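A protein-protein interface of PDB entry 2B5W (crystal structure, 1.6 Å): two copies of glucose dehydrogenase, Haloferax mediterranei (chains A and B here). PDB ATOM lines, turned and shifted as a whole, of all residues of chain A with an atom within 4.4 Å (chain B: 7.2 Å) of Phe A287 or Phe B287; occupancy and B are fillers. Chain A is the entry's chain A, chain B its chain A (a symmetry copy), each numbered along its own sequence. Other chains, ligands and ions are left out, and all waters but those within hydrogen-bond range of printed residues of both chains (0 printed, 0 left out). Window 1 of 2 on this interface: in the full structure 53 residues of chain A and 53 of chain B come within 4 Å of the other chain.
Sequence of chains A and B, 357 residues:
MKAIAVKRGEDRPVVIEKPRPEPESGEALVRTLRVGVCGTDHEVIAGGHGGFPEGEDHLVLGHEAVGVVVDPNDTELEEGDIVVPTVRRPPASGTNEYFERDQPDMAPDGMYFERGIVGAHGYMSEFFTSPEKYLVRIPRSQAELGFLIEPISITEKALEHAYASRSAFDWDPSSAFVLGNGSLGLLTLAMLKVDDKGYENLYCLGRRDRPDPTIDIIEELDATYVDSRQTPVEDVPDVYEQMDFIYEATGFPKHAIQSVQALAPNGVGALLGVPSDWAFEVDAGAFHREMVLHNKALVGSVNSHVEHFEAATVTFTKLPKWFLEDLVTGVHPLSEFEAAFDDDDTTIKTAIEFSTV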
ATOM      1  N   ILE A 257      16.851  22.694  -3.139  1.00  0.00           N
ATOM      2  CA  ILE A 257      15.913  23.651  -2.539  1.00  0.00           C
ATOM      3  C   ILE A 257      16.566  24.590  -1.549  1.00  0.00           C
ATOM      4  O   ILE A 257      16.371  25.798  -1.570  1.00  0.00           O
ATOM      5  CB  ILE A 257      14.773  22.888  -1.803  1.00  0.00           C
ATOM      6  CG1 ILE A 257      14.064  21.891  -2.728  1.00  0.00           C
ATOM      7  CG2 ILE A 257      13.813  23.880  -1.148  1.00  0.00           C
ATOM      8  CD1 ILE A 257      13.328  22.515  -3.895  1.00  0.00           C
ATOM      9  N   VAL A 260      19.222  27.804  -2.190  1.00  0.00           N
ATOM     10  CA  VAL A 260      18.746  29.171  -2.363  1.00  0.00           C
ATOM     11  C   VAL A 260      18.843  29.968  -1.063  1.00  0.00           C
ATOM     12  O   VAL A 260      19.133  31.147  -1.079  1.00  0.00           O
ATOM     13  CB  VAL A 260      17.302  29.144  -2.916  1.00  0.00           C
ATOM     14  CG1 VAL A 260      16.628  30.522  -2.862  1.00  0.00           C
ATOM     15  CG2 VAL A 260      17.365  28.631  -4.368  1.00  0.00           C
ATOM     16  N   GLN A 261      18.599  29.301   0.075  1.00  0.00           N
ATOM     17  CA  GLN A 261      18.686  29.974   1.357  1.00  0.00           C
ATOM     18  C   GLN A 261      20.124  30.206   1.811  1.00  0.00           C
ATOM     19  O   GLN A 261      20.378  31.137   2.563  1.00  0.00           O
ATOM     20  CB  GLN A 261      17.915  29.191   2.430  1.00  0.00           C
ATOM     21  CG  GLN A 261      16.440  28.933   2.097  1.00  0.00           C
ATOM     22  CD  GLN A 261      15.649  30.187   1.716  1.00  0.00           C
ATOM     23  OE1 GLN A 261      14.833  30.136   0.778  1.00  0.00           O
ATOM     24  NE2 GLN A 261      15.866  31.289   2.423  1.00  0.00           N
ATOM     25  N   ASP A 283       8.864  24.836   1.781  1.00  0.00           N
ATOM     26  CA  ASP A 283       8.385  26.197   1.787  1.00  0.00           C
ATOM     27  C   ASP A 283       8.756  26.828   0.416  1.00  0.00           C
ATOM     28  O   ASP A 283       9.785  27.490   0.282  1.00  0.00           O
ATOM     29  CB  ASP A 283       8.945  27.017   2.929  1.00  0.00           C
ATOM     30  CG  ASP A 283       8.178  28.303   3.143  1.00  0.00           C
ATOM     31  OD1 ASP A 283       7.622  28.857   2.163  1.00  0.00           O
ATOM     32  OD2 ASP A 283       8.071  28.852   4.252  1.00  0.00           O
ATOM     33  N   ALA A 284       7.882  26.595  -0.559  1.00  0.00           N
ATOM     34  CA  ALA A 284       8.047  27.081  -1.923  1.00  0.00           C
ATOM     35  C   ALA A 284       7.926  28.607  -1.982  1.00  0.00           C
ATOM     36  O   ALA A 284       8.558  29.250  -2.816  1.00  0.00           O
ATOM     37  CB  ALA A 284       7.021  26.428  -2.810  1.00  0.00           C
ATOM     38  N   GLY A 285       7.100  29.208  -1.125  1.00  0.00           N
ATOM     39  CA  GLY A 285       7.037  30.650  -1.013  1.00  0.00           C
ATOM     40  C   GLY A 285       8.373  31.277  -0.674  1.00  0.00           C
ATOM     41  O   GLY A 285       8.781  32.267  -1.299  1.00  0.00           O
ATOM     42  N   ALA A 286       9.060  30.713   0.321  1.00  0.00           N
ATOM     43  CA  ALA A 286      10.353  31.241   0.731  1.00  0.00           C
ATOM     44  C   ALA A 286      11.425  31.046  -0.359  1.00  0.00           C
ATOM     45  O   ALA A 286      12.252  31.916  -0.533  1.00  0.00           O
ATOM     46  CB  ALA A 286      10.821  30.586   2.058  1.00  0.00           C
ATOM     47  N   PHE A 287      11.395  29.897  -1.008  1.00  0.00           N
ATOM     48  CA  PHE A 287      12.276  29.569  -2.138  1.00  0.00           C
ATOM     49  C   PHE A 287      12.106  30.617  -3.231  1.00  0.00           C
ATOM     50  O   PHE A 287      13.051  31.260  -3.664  1.00  0.00           O
ATOM     51  CB  PHE A 287      11.918  28.176  -2.653  1.00  0.00           C
ATOM     52  CG  PHE A 287      12.547  27.817  -3.958  1.00  0.00           C
ATOM     53  CD1 PHE A 287      13.786  27.200  -3.993  1.00  0.00           C
ATOM     54  CD2 PHE A 287      11.902  28.089  -5.167  1.00  0.00           C
ATOM     55  CE1 PHE A 287      14.375  26.835  -5.209  1.00  0.00           C
ATOM     56  CE2 PHE A 287      12.505  27.752  -6.383  1.00  0.00           C
ATOM     57  CZ  PHE A 287      13.744  27.125  -6.395  1.00  0.00           C
ATOM     58  N   HIS A 288      10.861  30.803  -3.656  1.00  0.00           N
ATOM     59  CA  HIS A 288      10.503  31.694  -4.751  1.00  0.00           C
ATOM     60  C   HIS A 288      10.870  33.123  -4.426  1.00  0.00           C
ATOM     61  O   HIS A 288      11.556  33.773  -5.196  1.00  0.00           O
ATOM     62  CB  HIS A 288       8.996  31.537  -4.977  1.00  0.00           C
ATOM     63  CG  HIS A 288       8.437  32.267  -6.159  1.00  0.00           C
ATOM     64  ND1 HIS A 288       7.139  32.060  -6.579  1.00  0.00           N
ATOM     65  CD2 HIS A 288       8.963  33.190  -7.001  1.00  0.00           C
ATOM     66  CE1 HIS A 288       6.900  32.801  -7.649  1.00  0.00           C
ATOM     67  NE2 HIS A 288       7.993  33.492  -7.932  1.00  0.00           N
ATOM     68  N   ARG A 289      10.463  33.640  -3.261  1.00  0.00           N
ATOM     69  CA  ARG A 289      10.711  35.024  -2.920  1.00  0.00           C
ATOM     70  C   ARG A 289      12.225  35.361  -2.790  1.00  0.00           C
ATOM     71  O   ARG A 289      12.668  36.418  -3.200  1.00  0.00           O
ATOM     72  CB  ARG A 289       9.979  35.392  -1.610  1.00  0.00           C
ATOM     73  CG  ARG A 289      10.123  36.809  -1.218  1.00  0.00           C
ATOM     74  CD  ARG A 289       9.350  37.202   0.035  1.00  0.00           C
ATOM     75  NE  ARG A 289       9.952  36.609   1.235  1.00  0.00           N
ATOM     76  CZ  ARG A 289       9.537  35.507   1.849  1.00  0.00           C
ATOM     77  NH1 ARG A 289       8.472  34.831   1.427  1.00  0.00           N
ATOM     78  NH2 ARG A 289      10.198  35.083   2.917  1.00  0.00           N
ATOM     79  N   GLU A 290      12.981  34.454  -2.184  1.00  0.00           N
ATOM     80  CA  GLU A 290      14.413  34.649  -2.008  1.00  0.00           C
ATOM     81  C   GLU A 290      15.124  34.691  -3.355  1.00  0.00           C
ATOM     82  O   GLU A 290      16.025  35.500  -3.545  1.00  0.00           O
ATOM     83  CB  GLU A 290      14.966  33.528  -1.149  1.00  0.00           C
ATOM     84  CG  GLU A 290      16.433  33.703  -0.762  1.00  0.00           C
ATOM     85  CD  GLU A 290      16.737  35.015  -0.034  1.00  0.00           C
ATOM     86  OE1 GLU A 290      15.854  35.614   0.628  1.00  0.00           O
ATOM     87  OE2 GLU A 290      17.884  35.467  -0.103  1.00  0.00           O
ATOM     88  N   MET A 291      14.697  33.849  -4.298  1.00  0.00           N
ATOM     89  CA  MET A 291      15.298  33.909  -5.645  1.00  0.00           C
ATOM     90  C   MET A 291      15.118  35.272  -6.252  1.00  0.00           C
ATOM     91  O   MET A 291      16.005  35.855  -6.903  1.00  0.00           O
ATOM     92  CB  MET A 291      14.678  32.892  -6.589  1.00  0.00           C
ATOM     93  CG  MET A 291      14.985  31.474  -6.329  1.00  0.00           C
ATOM     94  SD  MET A 291      16.613  30.969  -6.915  1.00  0.00           S
ATOM     95  CE  MET A 291      16.538  31.146  -8.756  1.00  0.00           C
ATOM     96  N   LEU A 298      19.669  29.483 -10.213  1.00  0.00           N
ATOM     97  CA  LEU A 298      20.001  28.070 -10.185  1.00  0.00           C
ATOM     98  C   LEU A 298      20.174  27.615 -11.620  1.00  0.00           C
ATOM     99  O   LEU A 298      19.346  27.876 -12.466  1.00  0.00           O
ATOM    100  CB  LEU A 298      18.886  27.236  -9.558  1.00  0.00           C
ATOM    101  CG  LEU A 298      18.659  27.444  -8.073  1.00  0.00           C
ATOM    102  CD1 LEU A 298      17.437  26.620  -7.608  1.00  0.00           C
ATOM    103  CD2 LEU A 298      19.898  27.024  -7.282  1.00  0.00           C
ATOM    104  N   PRO B 253       3.699  30.671  -5.705  1.00  0.00           N
ATOM    105  CA  PRO B 253       4.858  29.770  -5.511  1.00  0.00           C
ATOM    106  C   PRO B 253       4.876  28.466  -6.285  1.00  0.00           C
ATOM    107  O   PRO B 253       5.939  28.008  -6.739  1.00  0.00           O
ATOM    108  CB  PRO B 253       4.839  29.519  -4.012  1.00  0.00           C
ATOM    109  CG  PRO B 253       4.258  30.753  -3.471  1.00  0.00           C
ATOM    110  CD  PRO B 253       3.177  31.149  -4.418  1.00  0.00           C
ATOM    111  N   ALA B 256       6.795  28.769  -9.584  1.00  0.00           N
ATOM    112  CA  ALA B 256       8.258  28.692  -9.547  1.00  0.00           C
ATOM    113  C   ALA B 256       8.721  27.237  -9.668  1.00  0.00           C
ATOM    114  O   ALA B 256       9.599  26.923 -10.461  1.00  0.00           O
ATOM    115  CB  ALA B 256       8.801  29.332  -8.287  1.00  0.00           C
ATOM    116  N   ILE B 257       8.074  26.345  -8.921  1.00  0.00           N
ATOM    117  CA  ILE B 257       8.419  24.918  -8.917  1.00  0.00           C
ATOM    118  C   ILE B 257       8.059  24.211 -10.205  1.00  0.00           C
ATOM    119  O   ILE B 257       8.842  23.468 -10.782  1.00  0.00           O
ATOM    120  CB  ILE B 257       7.686  24.197  -7.748  1.00  0.00           C
ATOM    121  CG1 ILE B 257       7.977  24.862  -6.397  1.00  0.00           C
ATOM    122  CG2 ILE B 257       8.015  22.705  -7.761  1.00  0.00           C
ATOM    123  CD1 ILE B 257       9.424  24.801  -5.952  1.00  0.00           C
ATOM    124  N   GLN B 258       6.842  24.456 -10.690  1.00  0.00           N
ATOM    125  CA  GLN B 258       6.349  23.730 -11.828  1.00  0.00           C
ATOM    126  C   GLN B 258       6.865  24.229 -13.147  1.00  0.00           C
ATOM    127  O   GLN B 258       6.813  23.495 -14.128  1.00  0.00           O
ATOM    128  CB  GLN B 258       4.814  23.720 -11.853  1.00  0.00           C
ATOM    129  CG  GLN B 258       4.208  22.956 -10.658  1.00  0.00           C
ATOM    130  CD  GLN B 258       4.725  21.516 -10.521  1.00  0.00           C
ATOM    131  OE1 GLN B 258       5.020  20.846 -11.512  1.00  0.00           O
ATOM    132  NE2 GLN B 258       4.813  21.037  -9.280  1.00  0.00           N
ATOM    133  N   SER B 259       7.398  25.454 -13.165  1.00  0.00           N
ATOM    134  CA  SER B 259       7.959  26.017 -14.389  1.00  0.00           C
ATOM    135  C   SER B 259       9.030  25.096 -14.931  1.00  0.00           C
ATOM    136  O   SER B 259       9.168  24.935 -16.123  1.00  0.00           O
ATOM    137  CB  SER B 259       8.555  27.410 -14.150  1.00  0.00           C
ATOM    138  OG  SER B 259       9.616  27.396 -13.200  1.00  0.00           O
ATOM    139  N   VAL B 260       9.799  24.480 -14.038  1.00  0.00           N
ATOM    140  CA  VAL B 260      10.863  23.579 -14.464  1.00  0.00           C
ATOM    141  C   VAL B 260      10.320  22.429 -15.309  1.00  0.00           C
ATOM    142  O   VAL B 260      10.962  21.987 -16.241  1.00  0.00           O
ATOM    143  CB  VAL B 260      11.629  23.069 -13.220  1.00  0.00           C
ATOM    144  CG1 VAL B 260      12.576  21.906 -13.552  1.00  0.00           C
ATOM    145  CG2 VAL B 260      12.418  24.257 -12.636  1.00  0.00           C
ATOM    146  N   GLN B 261       9.115  21.947 -14.972  1.00  0.00           N
ATOM    147  CA  GLN B 261       8.513  20.866 -15.730  1.00  0.00           C
ATOM    148  C   GLN B 261       7.945  21.325 -17.071  1.00  0.00           C
ATOM    149  O   GLN B 261       7.862  20.529 -17.996  1.00  0.00           O
ATOM    150  CB  GLN B 261       7.420  20.172 -14.906  1.00  0.00           C
ATOM    151  CG  GLN B 261       7.888  19.632 -13.549  1.00  0.00           C
ATOM    152  CD  GLN B 261       9.122  18.729 -13.619  1.00  0.00           C
ATOM    153  OE1 GLN B 261      10.011  18.839 -12.755  1.00  0.00           O
ATOM    154  NE2 GLN B 261       9.183  17.848 -14.609  1.00  0.00           N
ATOM    155  N   LEU B 271      11.954  34.626 -12.855  1.00  0.00           N
ATOM    156  CA  LEU B 271      11.007  34.724 -11.738  1.00  0.00           C
ATOM    157  C   LEU B 271      10.939  36.179 -11.308  1.00  0.00           C
ATOM    158  O   LEU B 271      11.980  36.786 -11.020  1.00  0.00           O
ATOM    159  CB  LEU B 271      11.427  33.823 -10.568  1.00  0.00           C
ATOM    160  CG  LEU B 271      11.634  32.351 -10.900  1.00  0.00           C
ATOM    161  CD1 LEU B 271      12.097  31.651  -9.643  1.00  0.00           C
ATOM    162  CD2 LEU B 271      10.362  31.700 -11.468  1.00  0.00           C
ATOM    163  N   PRO B 275       6.079  36.211  -3.490  1.00  0.00           N
ATOM    164  CA  PRO B 275       5.096  35.516  -2.631  1.00  0.00           C
ATOM    165  C   PRO B 275       5.444  35.524  -1.176  1.00  0.00           C
ATOM    166  O   PRO B 275       6.609  35.631  -0.819  1.00  0.00           O
ATOM    167  CB  PRO B 275       5.121  34.079  -3.133  1.00  0.00           C
ATOM    168  CG  PRO B 275       6.552  33.883  -3.687  1.00  0.00           C
ATOM    169  CD  PRO B 275       6.975  35.240  -4.140  1.00  0.00           C
ATOM    170  N   ASP B 277       5.540  33.296   2.418  1.00  0.00           N
ATOM    171  CA  ASP B 277       5.833  31.907   2.744  1.00  0.00           C
ATOM    172  C   ASP B 277       4.595  31.032   2.562  1.00  0.00           C
ATOM    173  O   ASP B 277       3.459  31.435   2.865  1.00  0.00           O
ATOM    174  CB  ASP B 277       6.345  31.774   4.188  1.00  0.00           C
ATOM    175  CG  ASP B 277       7.713  32.392   4.385  1.00  0.00           C
ATOM    176  OD1 ASP B 277       8.337  32.866   3.405  1.00  0.00           O
ATOM    177  OD2 ASP B 277       8.250  32.451   5.505  1.00  0.00           O
ATOM    178  N   TRP B 278       4.837  29.840   2.040  1.00  0.00           N
ATOM    179  CA  TRP B 278       3.811  28.858   1.773  1.00  0.00           C
ATOM    180  C   TRP B 278       4.470  27.493   1.577  1.00  0.00           C
ATOM    181  O   TRP B 278       5.220  27.292   0.627  1.00  0.00           O
ATOM    182  CB  TRP B 278       2.969  29.265   0.557  1.00  0.00           C
ATOM    183  CG  TRP B 278       1.810  28.340   0.277  1.00  0.00           C
ATOM    184  CD1 TRP B 278       1.213  27.477   1.154  1.00  0.00           C
ATOM    185  CD2 TRP B 278       1.123  28.188  -0.963  1.00  0.00           C
ATOM    186  NE1 TRP B 278       0.202  26.790   0.528  1.00  0.00           N
ATOM    187  CE2 TRP B 278       0.119  27.211  -0.772  1.00  0.00           C
ATOM    188  CE3 TRP B 278       1.248  28.782  -2.228  1.00  0.00           C
ATOM    189  CZ2 TRP B 278      -0.750  26.818  -1.795  1.00  0.00           C
ATOM    190  CZ3 TRP B 278       0.387  28.388  -3.243  1.00  0.00           C
ATOM    191  CH2 TRP B 278      -0.597  27.414  -3.020  1.00  0.00           C
ATOM    192  N   VAL B 282       6.158  19.025  -2.377  1.00  0.00           N
ATOM    193  CA  VAL B 282       6.845  19.214  -3.657  1.00  0.00           C
ATOM    194  C   VAL B 282       7.669  17.981  -3.980  1.00  0.00           C
ATOM    195  O   VAL B 282       8.388  17.486  -3.105  1.00  0.00           O
ATOM    196  CB  VAL B 282       7.802  20.415  -3.548  1.00  0.00           C
ATOM    197  CG1 VAL B 282       8.694  20.526  -4.782  1.00  0.00           C
ATOM    198  CG2 VAL B 282       7.004  21.704  -3.324  1.00  0.00           C
ATOM    199  N   ASP B 283       7.578  17.482  -5.208  1.00  0.00           N
ATOM    200  CA  ASP B 283       8.502  16.473  -5.668  1.00  0.00           C
ATOM    201  C   ASP B 283       9.833  17.191  -6.028  1.00  0.00           C
ATOM    202  O   ASP B 283      10.074  17.535  -7.186  1.00  0.00           O
ATOM    203  CB  ASP B 283       7.979  15.682  -6.847  1.00  0.00           C
ATOM    204  CG  ASP B 283       8.772  14.416  -7.087  1.00  0.00           C
ATOM    205  OD1 ASP B 283       9.988  14.386  -6.779  1.00  0.00           O
ATOM    206  OD2 ASP B 283       8.277  13.391  -7.583  1.00  0.00           O
ATOM    207  N   ALA B 284      10.657  17.384  -5.002  1.00  0.00           N
ATOM    208  CA  ALA B 284      11.948  18.051  -5.120  1.00  0.00           C
ATOM    209  C   ALA B 284      12.932  17.209  -5.938  1.00  0.00           C
ATOM    210  O   ALA B 284      13.793  17.750  -6.625  1.00  0.00           O
ATOM    211  CB  ALA B 284      12.493  18.323  -3.743  1.00  0.00           C
ATOM    212  N   GLY B 285      12.840  15.881  -5.861  1.00  0.00           N
ATOM    213  CA  GLY B 285      13.628  15.014  -6.711  1.00  0.00           C
ATOM    214  C   GLY B 285      13.409  15.271  -8.187  1.00  0.00           C
ATOM    215  O   GLY B 285      14.374  15.369  -8.960  1.00  0.00           O
ATOM    216  N   ALA B 286      12.143  15.376  -8.592  1.00  0.00           N
ATOM    217  CA  ALA B 286      11.821  15.618  -9.991  1.00  0.00           C
ATOM    218  C   ALA B 286      12.271  17.019 -10.450  1.00  0.00           C
ATOM    219  O   ALA B 286      12.715  17.156 -11.570  1.00  0.00           O
ATOM    220  CB  ALA B 286      10.300  15.439 -10.247  1.00  0.00           C
ATOM    221  N   PHE B 287      12.090  18.001  -9.587  1.00  0.00           N
ATOM    222  CA  PHE B 287      12.539  19.383  -9.810  1.00  0.00           C
ATOM    223  C   PHE B 287      14.041  19.390 -10.072  1.00  0.00           C
ATOM    224  O   PHE B 287      14.518  19.874 -11.087  1.00  0.00           O
ATOM    225  CB  PHE B 287      12.193  20.218  -8.579  1.00  0.00           C
ATOM    226  CG  PHE B 287      12.820  21.572  -8.551  1.00  0.00           C
ATOM    227  CD1 PHE B 287      12.171  22.657  -9.117  1.00  0.00           C
ATOM    228  CD2 PHE B 287      14.067  21.776  -7.955  1.00  0.00           C
ATOM    229  CE1 PHE B 287      12.737  23.936  -9.076  1.00  0.00           C
ATOM    230  CE2 PHE B 287      14.645  23.050  -7.941  1.00  0.00           C
ATOM    231  CZ  PHE B 287      13.973  24.126  -8.505  1.00  0.00           C
ATOM    232  N   HIS B 288      14.786  18.808  -9.139  1.00  0.00           N
ATOM    233  CA  HIS B 288      16.242  18.787  -9.160  1.00  0.00           C
ATOM    234  C   HIS B 288      16.752  18.053 -10.379  1.00  0.00           C
ATOM    235  O   HIS B 288      17.557  18.584 -11.125  1.00  0.00           O
ATOM    236  CB  HIS B 288      16.696  18.110  -7.864  1.00  0.00           C
ATOM    237  CG  HIS B 288      18.173  18.107  -7.616  1.00  0.00           C
ATOM    238  ND1 HIS B 288      18.694  17.699  -6.405  1.00  0.00           N
ATOM    239  CD2 HIS B 288      19.235  18.442  -8.389  1.00  0.00           C
ATOM    240  CE1 HIS B 288      20.013  17.813  -6.433  1.00  0.00           C
ATOM    241  NE2 HIS B 288      20.368  18.269  -7.624  1.00  0.00           N
ATOM    242  N   ARG B 289      16.271  16.832 -10.640  1.00  0.00           N
ATOM    243  CA  ARG B 289      16.772  16.041 -11.743  1.00  0.00           C
ATOM    244  C   ARG B 289      16.497  16.686 -13.133  1.00  0.00           C
ATOM    245  O   ARG B 289      17.329  16.638 -14.020  1.00  0.00           O
ATOM    246  CB  ARG B 289      16.173  14.619 -11.698  1.00  0.00           C
ATOM    247  CG  ARG B 289      16.681  13.718 -12.753  1.00  0.00           C
ATOM    248  CD  ARG B 289      16.149  12.291 -12.679  1.00  0.00           C
ATOM    249  NE  ARG B 289      14.729  12.236 -13.047  1.00  0.00           N
ATOM    250  CZ  ARG B 289      13.708  12.200 -12.199  1.00  0.00           C
ATOM    251  NH1 ARG B 289      13.893  12.180 -10.881  1.00  0.00           N
ATOM    252  NH2 ARG B 289      12.475  12.171 -12.685  1.00  0.00           N
ATOM    253  N   GLU B 290      15.306  17.248 -13.296  1.00  0.00           N
ATOM    254  CA  GLU B 290      14.931  17.890 -14.548  1.00  0.00           C
ATOM    255  C   GLU B 290      15.807  19.107 -14.817  1.00  0.00           C
ATOM    256  O   GLU B 290      16.209  19.330 -15.953  1.00  0.00           O
ATOM    257  CB  GLU B 290      13.469  18.292 -14.482  1.00  0.00           C
ATOM    258  CG  GLU B 290      12.913  18.838 -15.796  1.00  0.00           C
ATOM    259  CD  GLU B 290      13.061  17.884 -16.984  1.00  0.00           C
ATOM    260  OE1 GLU B 290      13.131  16.642 -16.819  1.00  0.00           O
ATOM    261  OE2 GLU B 290      13.097  18.369 -18.119  1.00  0.00           O
ATOM    262  N   MET B 291      16.134  19.869 -13.771  1.00  0.00           N
ATOM    263  CA  MET B 291      17.049  21.010 -13.967  1.00  0.00           C
ATOM    264  C   MET B 291      18.369  20.550 -14.520  1.00  0.00           C
ATOM    265  O   MET B 291      18.993  21.164 -15.406  1.00  0.00           O
ATOM    266  CB  MET B 291      17.320  21.750 -12.667  1.00  0.00           C
ATOM    267  CG  MET B 291      16.200  22.525 -12.101  1.00  0.00           C
ATOM    268  SD  MET B 291      15.943  24.115 -12.909  1.00  0.00           S
ATOM    269  CE  MET B 291      17.474  25.092 -12.550  1.00  0.00           C
ATOM    270  N   VAL B 292      18.890  19.455 -13.972  1.00  0.00           N
ATOM    271  CA  VAL B 292      20.207  19.011 -14.316  1.00  0.00           C
ATOM    272  C   VAL B 292      20.259  18.293 -15.651  1.00  0.00           C
ATOM    273  O   VAL B 292      21.030  18.664 -16.545  1.00  0.00           O
ATOM    274  CB  VAL B 292      20.740  18.061 -13.195  1.00  0.00           C
ATOM    275  CG1 VAL B 292      22.063  17.381 -13.599  1.00  0.00           C
ATOM    276  CG2 VAL B 292      20.889  18.847 -11.894  1.00  0.00           C
ATOM    277  N   LYS B 296      18.676  23.218 -17.510  1.00  0.00           N
ATOM    278  CA  LYS B 296      17.737  24.322 -17.344  1.00  0.00           C
ATOM    279  C   LYS B 296      18.215  25.331 -16.307  1.00  0.00           C
ATOM    280  O   LYS B 296      19.055  25.026 -15.448  1.00  0.00           O
ATOM    281  CB  LYS B 296      16.365  23.789 -16.955  1.00  0.00           C
ATOM    282  CG  LYS B 296      15.662  23.045 -18.054  1.00  0.00           C
ATOM    283  CD  LYS B 296      14.412  22.278 -17.582  1.00  0.00           C
ATOM    284  CE  LYS B 296      13.744  21.631 -18.756  1.00  0.00           C
ATOM    285  NZ  LYS B 296      12.462  20.968 -18.353  1.00  0.00           N
ATOM    286  N   LEU B 298      16.818  28.716 -13.612  1.00  0.00           N
ATOM    287  CA  LEU B 298      15.873  29.643 -13.017  1.00  0.00           C
ATOM    288  C   LEU B 298      16.656  30.855 -12.554  1.00  0.00           C
ATOM    289  O   LEU B 298      17.664  30.738 -11.891  1.00  0.00           O
ATOM    290  CB  LEU B 298      15.175  29.042 -11.799  1.00  0.00           C
ATOM    291  CG  LEU B 298      14.221  27.897 -12.082  1.00  0.00           C
ATOM    292  CD1 LEU B 298      13.680  27.324 -10.752  1.00  0.00           C
ATOM    293  CD2 LEU B 298      13.058  28.377 -12.951  1.00  0.00           C
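The backbone NH (N) of Gly A285 sits close to the side-chain carboxylate (OD1) of Asp A283 (3.3 Å).
OD1 of Asp A283 is in hydrogen-bond range of N of Ala A286, 3.0 Å away.
The backbone carbonyl oxygen of Met B291 lies within hydrogen-bond range of the backbone NH of Lys B296 (3.0 Å).
The side-chain amide oxygen (OE1) of Gln A261 lies close to the backbone carbonyl oxygen (O) of Ala A286 (3.4 Å).
The side-chain hydroxyl (OG) of Ser B259 sits at hydrogen-bond distance from the backbone carbonyl oxygen (O) of Ala B256.
Phe B287 touches its own counterpart, Phe A287.
Met A291 touches Leu B298, and with the chains exchanged Leu A298 touches Met B291.
Leu A298 touches its own counterpart, Leu B298.
Of the 17 pairs that touch across the chains among the printed residues, 4 have their exchanged pair printed and touching as well.
Of the 13 printed residues of chain A, 9 touch a printed residue of chain B.
Hydrophobic or aromatic side chains of chain A that line the printed part of chain B: Ala A284, Ala A286, Phe A287, His A288, Met A291 and Leu A298.
Of the 24 printed residues of chain B, 8 touch a printed residue of chain A.
Printed residues of chain B that touch a printed residue of chain A: Pro B253, Ala B256, Pro B275, Asp B277, Trp B278, Phe B287, Met B291 and Leu B298.
Hydrophobic or aromatic side chains of chain B within 4 Å of the printed part of chain A: Pro B253, Ala B256, Pro B275, Phe B287, Met B291 and Leu B298.
Of chain B, only Phe B287 (3.7 Å) comes within 4 Å of Phe A287.
Of the printed residues of chain B, Gly A285 touches Pro B253 (3.7 Å), Pro B275 (3.6 Å) and Trp B278 (3.2 Å).
Of the printed residues of chain B, Met A291 touches Leu B298.
Gln B258 touches none of the printed residues of chain A.
Ala B286 touches none of the printed residues of chain A.
The nearest residue of chain B that does not touch Phe A287 is Ile B257 (4.2 Å).
The nearest residue of chain A that does not touch Phe B287 is Ile A257 (4.2 Å).
The nearest printed residue of chain B that does not touch Asp A283 is Val B282 (6.3 Å).
Among the printed residues, pairs that only touch across the chains: Leu A298 with Met B291 (3.4 Å), Met A291 with Leu B298 (3.4 Å), Asp A283 with Asp B277 (3.4 Å), His A288 with Pro B253 (3.4 Å), His A288 with Pro B275 (3.5 Å), His A288 with Ala B256 (3.6 Å), Ala A286 with Asp B277 (3.6 Å), Gly A285 with Pro B275 (3.6 Å), Phe A287 with Phe B287 (3.7 Å), Gly A285 with Pro B253 (3.7 Å) and Ala A284 with Pro B253 (3.8 Å).
NH1 of Arg A289 is in salt-bridge range of OD1 of Asp B277 (2.8 Å).
O of Trp B278 is in hydrogen-bond range of N of Ala A284, at 3.0 Å.
The backbone carbonyl oxygen (O) of Leu B298 sits at hydrogen-bond distance from the backbone NH (N) of Leu A298, at 2.9 Å.
The backbone carbonyl oxygen (O) of Trp B278 lies within hydrogen-bond range of the backbone NH (N) of Gly A285, at 3.2 Å.
NH1 of Arg A289 is in hydrogen-bond range of O of Pro B275, 3.0 Å away.
N of Trp B278 sits at hydrogen-bond distance from OD1 of Asp A283, at 3.0 Å.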
